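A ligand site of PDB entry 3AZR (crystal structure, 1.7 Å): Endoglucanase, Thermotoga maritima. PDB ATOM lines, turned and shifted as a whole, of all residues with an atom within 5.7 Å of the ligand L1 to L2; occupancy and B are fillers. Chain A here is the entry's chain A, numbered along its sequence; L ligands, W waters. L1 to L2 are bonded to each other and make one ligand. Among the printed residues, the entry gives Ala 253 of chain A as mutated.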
ATOM      1  N   ASN A  20     -17.983 -21.716  17.653  1.00  0.00           N
ATOM      2  CA  ASN A  20     -17.502 -21.740  19.033  1.00  0.00           C
ATOM      3  C   ASN A  20     -18.586 -21.138  19.933  1.00  0.00           C
ATOM      4  O   ASN A  20     -18.321 -20.525  20.950  1.00  0.00           O
ATOM      5  CB  ASN A  20     -16.145 -21.018  19.186  1.00  0.00           C
ATOM      6  CG  ASN A  20     -14.962 -21.953  18.906  1.00  0.00           C
ATOM      7  OD1 ASN A  20     -13.802 -21.586  19.050  1.00  0.00           O
ATOM      8  ND2 ASN A  20     -15.263 -23.198  18.540  1.00  0.00           N
ATOM      9  N   GLU A  23     -22.420 -24.860  19.396  1.00  0.00           N
ATOM     10  CA  GLU A  23     -21.949 -26.225  19.189  1.00  0.00           C
ATOM     11  C   GLU A  23     -20.987 -26.703  20.306  1.00  0.00           C
ATOM     12  O   GLU A  23     -20.568 -27.841  20.355  1.00  0.00           O
ATOM     13  CB  GLU A  23     -21.392 -26.405  17.740  1.00  0.00           C
ATOM     14  CG  GLU A  23     -19.929 -26.056  17.545  1.00  0.00           C
ATOM     15  CD  GLU A  23     -19.713 -24.565  17.460  1.00  0.00           C
ATOM     16  OE1 GLU A  23     -20.562 -23.784  17.932  1.00  0.00           O
ATOM     17  OE2 GLU A  23     -18.663 -24.170  16.881  1.00  0.00           O
ATOM     18  N   TRP A  30     -16.848 -22.267  24.672  1.00  0.00           N
ATOM     19  CA  TRP A  30     -15.758 -22.162  23.734  1.00  0.00           C
ATOM     20  C   TRP A  30     -15.463 -20.702  23.353  1.00  0.00           C
ATOM     21  O   TRP A  30     -14.843 -20.440  22.349  1.00  0.00           O
ATOM     22  CB  TRP A  30     -16.051 -23.016  22.504  1.00  0.00           C
ATOM     23  CG  TRP A  30     -15.965 -24.525  22.803  1.00  0.00           C
ATOM     24  CD1 TRP A  30     -15.695 -25.147  24.031  1.00  0.00           C
ATOM     25  CD2 TRP A  30     -16.225 -25.591  21.893  1.00  0.00           C
ATOM     26  NE1 TRP A  30     -15.788 -26.512  23.905  1.00  0.00           N
ATOM     27  CE2 TRP A  30     -16.106 -26.811  22.611  1.00  0.00           C
ATOM     28  CE3 TRP A  30     -16.553 -25.633  20.522  1.00  0.00           C
ATOM     29  CZ2 TRP A  30     -16.287 -28.061  22.001  1.00  0.00           C
ATOM     30  CZ3 TRP A  30     -16.740 -26.860  19.931  1.00  0.00           C
ATOM     31  CH2 TRP A  30     -16.599 -28.064  20.663  1.00  0.00           C
ATOM     32  N   ARG A  51     -24.525 -19.116   9.259  1.00  0.00           N
ATOM     33  CA  ARG A  51     -24.627 -20.541   9.538  1.00  0.00           C
ATOM     34  C   ARG A  51     -24.444 -20.702  11.037  1.00  0.00           C
ATOM     35  O   ARG A  51     -23.496 -20.135  11.645  1.00  0.00           O
ATOM     36  CB  ARG A  51     -23.584 -21.356   8.763  1.00  0.00           C
ATOM     37  CG  ARG A  51     -23.620 -22.869   9.066  1.00  0.00           C
ATOM     38  CD  ARG A  51     -22.843 -23.674   7.922  1.00  0.00           C
ATOM     39  NE  ARG A  51     -22.810 -25.127   8.243  1.00  0.00           N
ATOM     40  CZ  ARG A  51     -21.868 -25.716   8.967  1.00  0.00           C
ATOM     41  NH1 ARG A  51     -20.858 -25.011   9.491  1.00  0.00           N
ATOM     42  NH2 ARG A  51     -21.862 -27.032   9.121  1.00  0.00           N
ATOM     43  N   HIS A  95     -24.632 -30.538  14.983  1.00  0.00           N
ATOM     44  CA  HIS A  95     -23.195 -30.432  15.009  1.00  0.00           C
ATOM     45  C   HIS A  95     -22.579 -31.130  16.302  1.00  0.00           C
ATOM     46  O   HIS A  95     -23.131 -31.082  17.243  1.00  0.00           O
ATOM     47  CB  HIS A  95     -22.843 -28.960  15.003  1.00  0.00           C
ATOM     48  CG  HIS A  95     -21.505 -28.550  14.386  1.00  0.00           C
ATOM     49  ND1 HIS A  95     -21.396 -27.751  13.284  1.00  0.00           N
ATOM     50  CD2 HIS A  95     -20.255 -28.743  14.818  1.00  0.00           C
ATOM     51  CE1 HIS A  95     -20.116 -27.503  13.056  1.00  0.00           C
ATOM     52  NE2 HIS A  95     -19.423 -28.066  13.986  1.00  0.00           N
ATOM     53  N   HIS A  96     -21.421 -31.763  16.101  1.00  0.00           N
ATOM     54  CA  HIS A  96     -20.765 -32.480  17.193  1.00  0.00           C
ATOM     55  C   HIS A  96     -21.641 -33.499  17.914  1.00  0.00           C
ATOM     56  O   HIS A  96     -21.678 -33.534  19.153  1.00  0.00           O
ATOM     57  CB  HIS A  96     -20.129 -31.493  18.213  1.00  0.00           C
ATOM     58  CG  HIS A  96     -18.987 -30.720  17.619  1.00  0.00           C
ATOM     59  ND1 HIS A  96     -18.750 -29.383  17.891  1.00  0.00           N
ATOM     60  CD2 HIS A  96     -18.048 -31.099  16.733  1.00  0.00           C
ATOM     61  CE1 HIS A  96     -17.721 -28.975  17.177  1.00  0.00           C
ATOM     62  NE2 HIS A  96     -17.265 -29.991  16.464  1.00  0.00           N
ATOM     63  N   ASN A 135     -23.402 -32.106  10.408  1.00  0.00           N
ATOM     64  CA  ASN A 135     -22.062 -31.566  10.172  1.00  0.00           C
ATOM     65  C   ASN A 135     -21.015 -32.663  10.205  1.00  0.00           C
ATOM     66  O   ASN A 135     -20.945 -33.430  11.149  1.00  0.00           O
ATOM     67  CB  ASN A 135     -21.689 -30.603  11.295  1.00  0.00           C
ATOM     68  CG  ASN A 135     -20.310 -29.986  11.118  1.00  0.00           C
ATOM     69  OD1 ASN A 135     -20.114 -29.186  10.218  1.00  0.00           O
ATOM     70  ND2 ASN A 135     -19.376 -30.346  11.995  1.00  0.00           N
ATOM     71  N   GLU A 136     -20.191 -32.672   9.168  1.00  0.00           N
ATOM     72  CA  GLU A 136     -19.044 -33.592   9.031  1.00  0.00           C
ATOM     73  C   GLU A 136     -19.123 -35.046   9.508  1.00  0.00           C
ATOM     74  O   GLU A 136     -18.457 -35.431  10.472  1.00  0.00           O
ATOM     75  CB  GLU A 136     -17.822 -32.909   9.661  1.00  0.00           C
ATOM     76  CG  GLU A 136     -17.509 -31.574   8.973  1.00  0.00           C
ATOM     77  CD  GLU A 136     -16.229 -30.862   9.448  1.00  0.00           C
ATOM     78  OE1 GLU A 136     -15.568 -31.296  10.411  1.00  0.00           O
ATOM     79  OE2 GLU A 136     -15.881 -29.841   8.832  1.00  0.00           O
ATOM     80  N   HIS A 196     -16.813 -28.668   3.114  1.00  0.00           N
ATOM     81  CA  HIS A 196     -15.974 -27.776   3.889  1.00  0.00           C
ATOM     82  C   HIS A 196     -14.588 -27.821   3.227  1.00  0.00           C
ATOM     83  O   HIS A 196     -14.140 -28.890   2.788  1.00  0.00           O
ATOM     84  CB  HIS A 196     -15.978 -28.249   5.360  1.00  0.00           C
ATOM     85  CG  HIS A 196     -17.354 -28.208   5.956  1.00  0.00           C
ATOM     86  ND1 HIS A 196     -17.681 -28.765   7.180  1.00  0.00           N
ATOM     87  CD2 HIS A 196     -18.496 -27.668   5.463  1.00  0.00           C
ATOM     88  CE1 HIS A 196     -18.958 -28.552   7.415  1.00  0.00           C
ATOM     89  NE2 HIS A 196     -19.472 -27.883   6.396  1.00  0.00           N
ATOM     90  N   TYR A 198     -10.606 -26.797   3.733  1.00  0.00           N
ATOM     91  CA  TYR A 198      -9.562 -26.302   4.600  1.00  0.00           C
ATOM     92  C   TYR A 198      -8.218 -26.717   4.057  1.00  0.00           C
ATOM     93  O   TYR A 198      -7.242 -26.737   4.793  1.00  0.00           O
ATOM     94  CB  TYR A 198      -9.767 -26.902   5.979  1.00  0.00           C
ATOM     95  CG  TYR A 198     -10.954 -26.321   6.716  1.00  0.00           C
ATOM     96  CD1 TYR A 198     -10.898 -25.039   7.229  1.00  0.00           C
ATOM     97  CD2 TYR A 198     -12.077 -27.079   6.984  1.00  0.00           C
ATOM     98  CE1 TYR A 198     -11.902 -24.519   8.030  1.00  0.00           C
ATOM     99  CE2 TYR A 198     -13.110 -26.574   7.779  1.00  0.00           C
ATOM    100  CZ  TYR A 198     -13.007 -25.304   8.300  1.00  0.00           C
ATOM    101  OH  TYR A 198     -14.003 -24.831   9.132  1.00  0.00           O
ATOM    102  N   HIS A 205      -4.842 -25.353   9.568  1.00  0.00           N
ATOM    103  CA  HIS A 205      -4.889 -25.931  10.871  1.00  0.00           C
ATOM    104  C   HIS A 205      -3.605 -25.944  11.667  1.00  0.00           C
ATOM    105  O   HIS A 205      -3.505 -26.507  12.670  1.00  0.00           O
ATOM    106  CB  HIS A 205      -5.610 -27.298  10.820  1.00  0.00           C
ATOM    107  CG  HIS A 205      -7.096 -27.223  10.680  1.00  0.00           C
ATOM    108  ND1 HIS A 205      -7.743 -26.812   9.571  1.00  0.00           N
ATOM    109  CD2 HIS A 205      -8.037 -27.510  11.568  1.00  0.00           C
ATOM    110  CE1 HIS A 205      -9.030 -26.848   9.786  1.00  0.00           C
ATOM    111  NE2 HIS A 205      -9.224 -27.224  11.006  1.00  0.00           N
ATOM    112  N   TRP A 210      -6.754 -28.530  18.932  1.00  0.00           N
ATOM    113  CA  TRP A 210      -7.612 -29.714  18.938  1.00  0.00           C
ATOM    114  C   TRP A 210      -7.242 -30.741  17.869  1.00  0.00           C
ATOM    115  O   TRP A 210      -7.955 -31.734  17.687  1.00  0.00           O
ATOM    116  CB  TRP A 210      -9.093 -29.285  18.776  1.00  0.00           C
ATOM    117  CG  TRP A 210      -9.403 -28.577  17.483  1.00  0.00           C
ATOM    118  CD1 TRP A 210      -9.922 -29.120  16.354  1.00  0.00           C
ATOM    119  CD2 TRP A 210      -9.092 -27.205  17.152  1.00  0.00           C
ATOM    120  NE1 TRP A 210      -9.965 -28.193  15.337  1.00  0.00           N
ATOM    121  CE2 TRP A 210      -9.439 -27.012  15.795  1.00  0.00           C
ATOM    122  CE3 TRP A 210      -8.550 -26.142  17.867  1.00  0.00           C
ATOM    123  CZ2 TRP A 210      -9.261 -25.786  15.130  1.00  0.00           C
ATOM    124  CZ3 TRP A 210      -8.377 -24.930  17.211  1.00  0.00           C
ATOM    125  CH2 TRP A 210      -8.729 -24.759  15.851  1.00  0.00           C
ATOM    126  N   VAL A 211      -6.144 -30.508  17.160  1.00  0.00           N
ATOM    127  CA  VAL A 211      -5.712 -31.438  16.127  1.00  0.00           C
ATOM    128  C   VAL A 211      -4.371 -32.023  16.479  1.00  0.00           C
ATOM    129  O   VAL A 211      -3.378 -31.308  16.606  1.00  0.00           O
ATOM    130  CB  VAL A 211      -5.619 -30.757  14.755  1.00  0.00           C
ATOM    131  CG1 VAL A 211      -5.133 -31.771  13.701  1.00  0.00           C
ATOM    132  CG2 VAL A 211      -6.983 -30.188  14.388  1.00  0.00           C
ATOM    133  N   ALA A 253     -18.117 -24.146   5.245  1.00  0.00           N
ATOM    134  CA  ALA A 253     -17.084 -23.752   6.206  1.00  0.00           C
ATOM    135  C   ALA A 253     -15.711 -23.786   5.511  1.00  0.00           C
ATOM    136  O   ALA A 253     -15.401 -24.763   4.808  1.00  0.00           O
ATOM    137  CB  ALA A 253     -17.075 -24.681   7.428  1.00  0.00           C
ATOM    138  N   TRP A 286     -15.511 -19.662   8.047  1.00  0.00           N
ATOM    139  CA  TRP A 286     -15.333 -20.172   9.413  1.00  0.00           C
ATOM    140  C   TRP A 286     -14.169 -19.338   9.986  1.00  0.00           C
ATOM    141  O   TRP A 286     -13.038 -19.527   9.532  1.00  0.00           O
ATOM    142  CB  TRP A 286     -14.922 -21.632   9.422  1.00  0.00           C
ATOM    143  CG  TRP A 286     -14.838 -22.221  10.824  1.00  0.00           C
ATOM    144  CD1 TRP A 286     -13.742 -22.302  11.642  1.00  0.00           C
ATOM    145  CD2 TRP A 286     -15.944 -22.707  11.574  1.00  0.00           C
ATOM    146  NE1 TRP A 286     -14.098 -22.831  12.881  1.00  0.00           N
ATOM    147  CE2 TRP A 286     -15.455 -23.069  12.865  1.00  0.00           C
ATOM    148  CE3 TRP A 286     -17.306 -22.862  11.299  1.00  0.00           C
ATOM    149  CZ2 TRP A 286     -16.287 -23.586  13.871  1.00  0.00           C
ATOM    150  CZ3 TRP A 286     -18.121 -23.372  12.292  1.00  0.00           C
ATOM    151  CH2 TRP A 286     -17.621 -23.729  13.553  1.00  0.00           C
ATOM    152  N   GLU A 287     -14.417 -18.442  10.937  1.00  0.00           N
ATOM    153  CA  GLU A 287     -15.740 -18.126  11.486  1.00  0.00           C
ATOM    154  C   GLU A 287     -15.790 -16.667  11.934  1.00  0.00           C
ATOM    155  O   GLU A 287     -14.796 -15.928  11.772  1.00  0.00           O
ATOM    156  CB  GLU A 287     -16.167 -19.112  12.589  1.00  0.00           C
ATOM    157  CG  GLU A 287     -15.076 -19.678  13.483  1.00  0.00           C
ATOM    158  CD  GLU A 287     -14.423 -18.649  14.381  1.00  0.00           C
ATOM    159  OE1 GLU A 287     -15.057 -17.635  14.722  1.00  0.00           O
ATOM    160  OE2 GLU A 287     -13.254 -18.854  14.770  1.00  0.00           O
ATOM    161  N   SER A 290     -13.974 -15.873  16.657  1.00  0.00           N
ATOM    162  CA  SER A 290     -13.188 -16.645  17.597  1.00  0.00           C
ATOM    163  C   SER A 290     -11.787 -16.889  17.025  1.00  0.00           C
ATOM    164  O   SER A 290     -11.228 -15.974  16.410  1.00  0.00           O
ATOM    165  CB  SER A 290     -13.950 -17.953  17.948  1.00  0.00           C
ATOM    166  OG  SER A 290     -13.245 -18.759  18.836  1.00  0.00           O
ATOM    167  N   PHE A 292     -10.655 -18.266  14.398  1.00  0.00           N
ATOM    168  CA  PHE A 292     -10.514 -18.069  12.957  1.00  0.00           C
ATOM    169  C   PHE A 292     -11.201 -16.737  12.636  1.00  0.00           C
ATOM    170  O   PHE A 292     -11.403 -16.399  11.478  1.00  0.00           O
ATOM    171  CB  PHE A 292     -11.266 -19.152  12.164  1.00  0.00           C
ATOM    172  CG  PHE A 292     -10.611 -20.513  12.139  1.00  0.00           C
ATOM    173  CD1 PHE A 292     -10.042 -20.995  10.951  1.00  0.00           C
ATOM    174  CD2 PHE A 292     -10.666 -21.367  13.243  1.00  0.00           C
ATOM    175  CE1 PHE A 292      -9.564 -22.311  10.854  1.00  0.00           C
ATOM    176  CE2 PHE A 292     -10.176 -22.688  13.167  1.00  0.00           C
ATOM    177  CZ  PHE A 292      -9.625 -23.164  11.967  1.00  0.00           C
HETATM  178  C1  LIG L   1     -14.999 -27.707  10.810  1.00  0.00           C
HETATM  179  C2  LIG L   1     -15.767 -28.215  12.039  1.00  0.00           C
HETATM  180  C3  LIG L   1     -15.728 -27.145  13.127  1.00  0.00           C
HETATM  181  C4  LIG L   1     -14.277 -26.834  13.467  1.00  0.00           C
HETATM  182  C5  LIG L   1     -13.627 -26.311  12.196  1.00  0.00           C
HETATM  183  C6  LIG L   1     -12.150 -25.961  12.468  1.00  0.00           C
HETATM  184  O1  LIG L   1     -15.682 -26.591  10.225  1.00  0.00           O
HETATM  185  O2  LIG L   1     -17.123 -28.448  11.662  1.00  0.00           O
HETATM  186  O3  LIG L   1     -16.418 -27.582  14.308  1.00  0.00           O
HETATM  187  O4  LIG L   1     -14.235 -25.784  14.450  1.00  0.00           O
HETATM  188  O5  LIG L   1     -13.666 -27.314  11.165  1.00  0.00           O
HETATM  189  O6  LIG L   1     -11.428 -27.168  12.722  1.00  0.00           O
HETATM  190  C1  LG2 L   2     -13.103 -24.752  16.268  1.00  0.00           C
HETATM  191  C2  LG2 L   2     -12.186 -25.006  17.466  1.00  0.00           C
HETATM  192  C3  LG2 L   2     -12.796 -26.106  18.331  1.00  0.00           C
HETATM  193  C4  LG2 L   2     -13.066 -27.347  17.469  1.00  0.00           C
HETATM  194  C5  LG2 L   2     -13.698 -28.441  18.331  1.00  0.00           C
HETATM  195  C6  LG2 L   2     -13.327 -26.062  15.511  1.00  0.00           C
HETATM  196  O1  LG2 L   2     -12.595 -23.749  15.374  1.00  0.00           O
HETATM  197  O2  LG2 L   2     -12.101 -23.832  18.280  1.00  0.00           O
HETATM  198  O3  LG2 L   2     -11.892 -26.434  19.391  1.00  0.00           O
HETATM  199  O4  LG2 L   2     -13.958 -27.006  16.392  1.00  0.00           O
HETATM  200  O5  LG2 L   2     -13.852 -29.624  17.532  1.00  0.00           O
HETATM  201  C1  LG3 L   3     -11.507 -31.212  12.162  1.00  0.00           C
HETATM  202  C2  LG3 L   3     -10.316 -31.782  12.931  1.00  0.00           C
HETATM  203  C3  LG3 L   3      -9.971 -33.166  12.388  1.00  0.00           C
HETATM  204  C4  LG3 L   3      -9.741 -33.084  10.879  1.00  0.00           C
HETATM  205  C5  LG3 L   3      -9.430 -34.483  10.338  1.00  0.00           C
HETATM  206  C6  LG3 L   3     -11.205 -31.226  10.657  1.00  0.00           C
HETATM  207  O1  LG3 L   3     -12.341 -30.729   9.928  1.00  0.00           O
HETATM  208  O2  LG3 L   3     -11.751 -29.867  12.594  1.00  0.00           O
HETATM  209  O3  LG3 L   3     -10.653 -31.875  14.321  1.00  0.00           O
HETATM  210  O4  LG3 L   3      -8.786 -33.660  13.029  1.00  0.00           O
HETATM  211  O5  LG3 L   3     -10.927 -32.562  10.236  1.00  0.00           O
HETATM  212  O6  LG3 L   3      -9.232 -34.418   8.916  1.00  0.00           O
HETATM  213  O   HOH W   1     -18.435 -26.503  10.276  1.00  0.00           O
HETATM  214  O   HOH W   2     -12.631 -27.275  21.614  1.00  0.00           O
HETATM  215  O   HOH W   3     -10.558 -21.265  17.915  1.00  0.00           O
HETATM  216  O   HOH W   4     -14.084 -30.403  14.764  1.00  0.00           O
HETATM  217  O   HOH W   5     -16.823 -26.146  16.601  1.00  0.00           O
HETATM  218  O   HOH W   6     -12.666 -21.310  15.984  1.00  0.00           O
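OH of Tyr 198 sits at hydrogen-bond distance from O1 of LIG L1 (2.7 Å).
A ring nitrogen (NE2) of His 205 is in hydrogen-bond range of an oxygen (O6) of LIG L1 (2.8 Å).
O2 of LG2 L2 sits at hydrogen-bond distance from OD1 of Asn 20.
The side-chain amide nitrogen (ND2) of Asn 135 lies within hydrogen-bond range of an oxygen (O2) of LIG L1, at 3.0 Å.
The side-chain carboxylate (OE2) of Glu 136 sits close to an oxygen (O2) of LIG L1 (3.4 Å).
The indole nitrogen (NE1) of Trp 286 lies within hydrogen-bond range of an oxygen (O1) of LG2 L2 (3.1 Å).
An oxygen (O3) of LIG L1 sits at hydrogen-bond distance from a ring nitrogen (NE2) of His 95, at 3.1 Å.
An oxygen (O6) of LIG L1 sits at hydrogen-bond distance from the indole nitrogen of Trp 210.
A ring nitrogen (NE2) of His 96 lies within hydrogen-bond range of an oxygen (O3) of LIG L1, at 3.3 Å.
O1 of LG3 L3 sits at hydrogen-bond distance from OE1 of Glu 136 (3.3 Å).
The side-chain carboxylate of Glu 23 is in hydrogen-bond range of the backbone NH of Asn 20 (2.7 Å).
The side-chain amide oxygen of Asn 20 lies within hydrogen-bond range of the side-chain hydroxyl of Ser 290, at 2.9 Å.
A ring nitrogen (NE2) of His 95 lies within hydrogen-bond range of the side-chain amide nitrogen (ND2) of Asn 135 (3.0 Å).
OD1 of Asn 135 lies within hydrogen-bond range of NH2 of Arg 51, 3.0 Å away.
The side-chain carboxylate (OE2) of Glu 136 lies within hydrogen-bond range of a ring nitrogen (ND1) of His 196, 2.7 Å away.
A ring nitrogen (ND1) of His 96 sits at hydrogen-bond distance from the backbone carbonyl oxygen of Glu 23 (3.4 Å).
N of Phe 292 lies within hydrogen-bond range of OE2 of Glu 287, 2.7 Å away.
Water W6 lies within hydrogen-bond range of O1 of LG2 L2 (2.5 Å), OE2 of Glu 287 (2.8 Å) and OD1 of Asn 20 (3.3 Å).
Water W1 lies within hydrogen-bond range of O2 of LIG L1 (2.7 Å), NH1 of Arg 51 (3.0 Å) and OD1 of Asn 135 (3.2 Å).
Water W5 bridges OE2 of Glu 23 and O3 of LIG L1.
Water W4 lies within hydrogen-bond range of an oxygen (O5) of LG2 L2 and an oxygen (O2) of LG3 L3.
Water W3 bridges an oxygen (O2) of LG2 L2 (3.0 Å) and the side-chain amide oxygen of Asn 20 (3.5 Å).
Residues that only touch the ligand L1 to L2: Trp 30, Ala 253 and Phe 292.
Hydrophobic or aromatic side chains that line the ligand L1 to L2: Trp 30, His 95, His 96, Tyr 198, His 205, Trp 210, Ala 253, Trp 286 and Phe 292.
The nearest printed residue that does not touch the ligand L1 to L2 is His 196 (4.2 Å).
An oxygen (O2) of LG3 L3 is in hydrogen-bond range of an oxygen (O6) of LIG L1 (2.7 Å).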
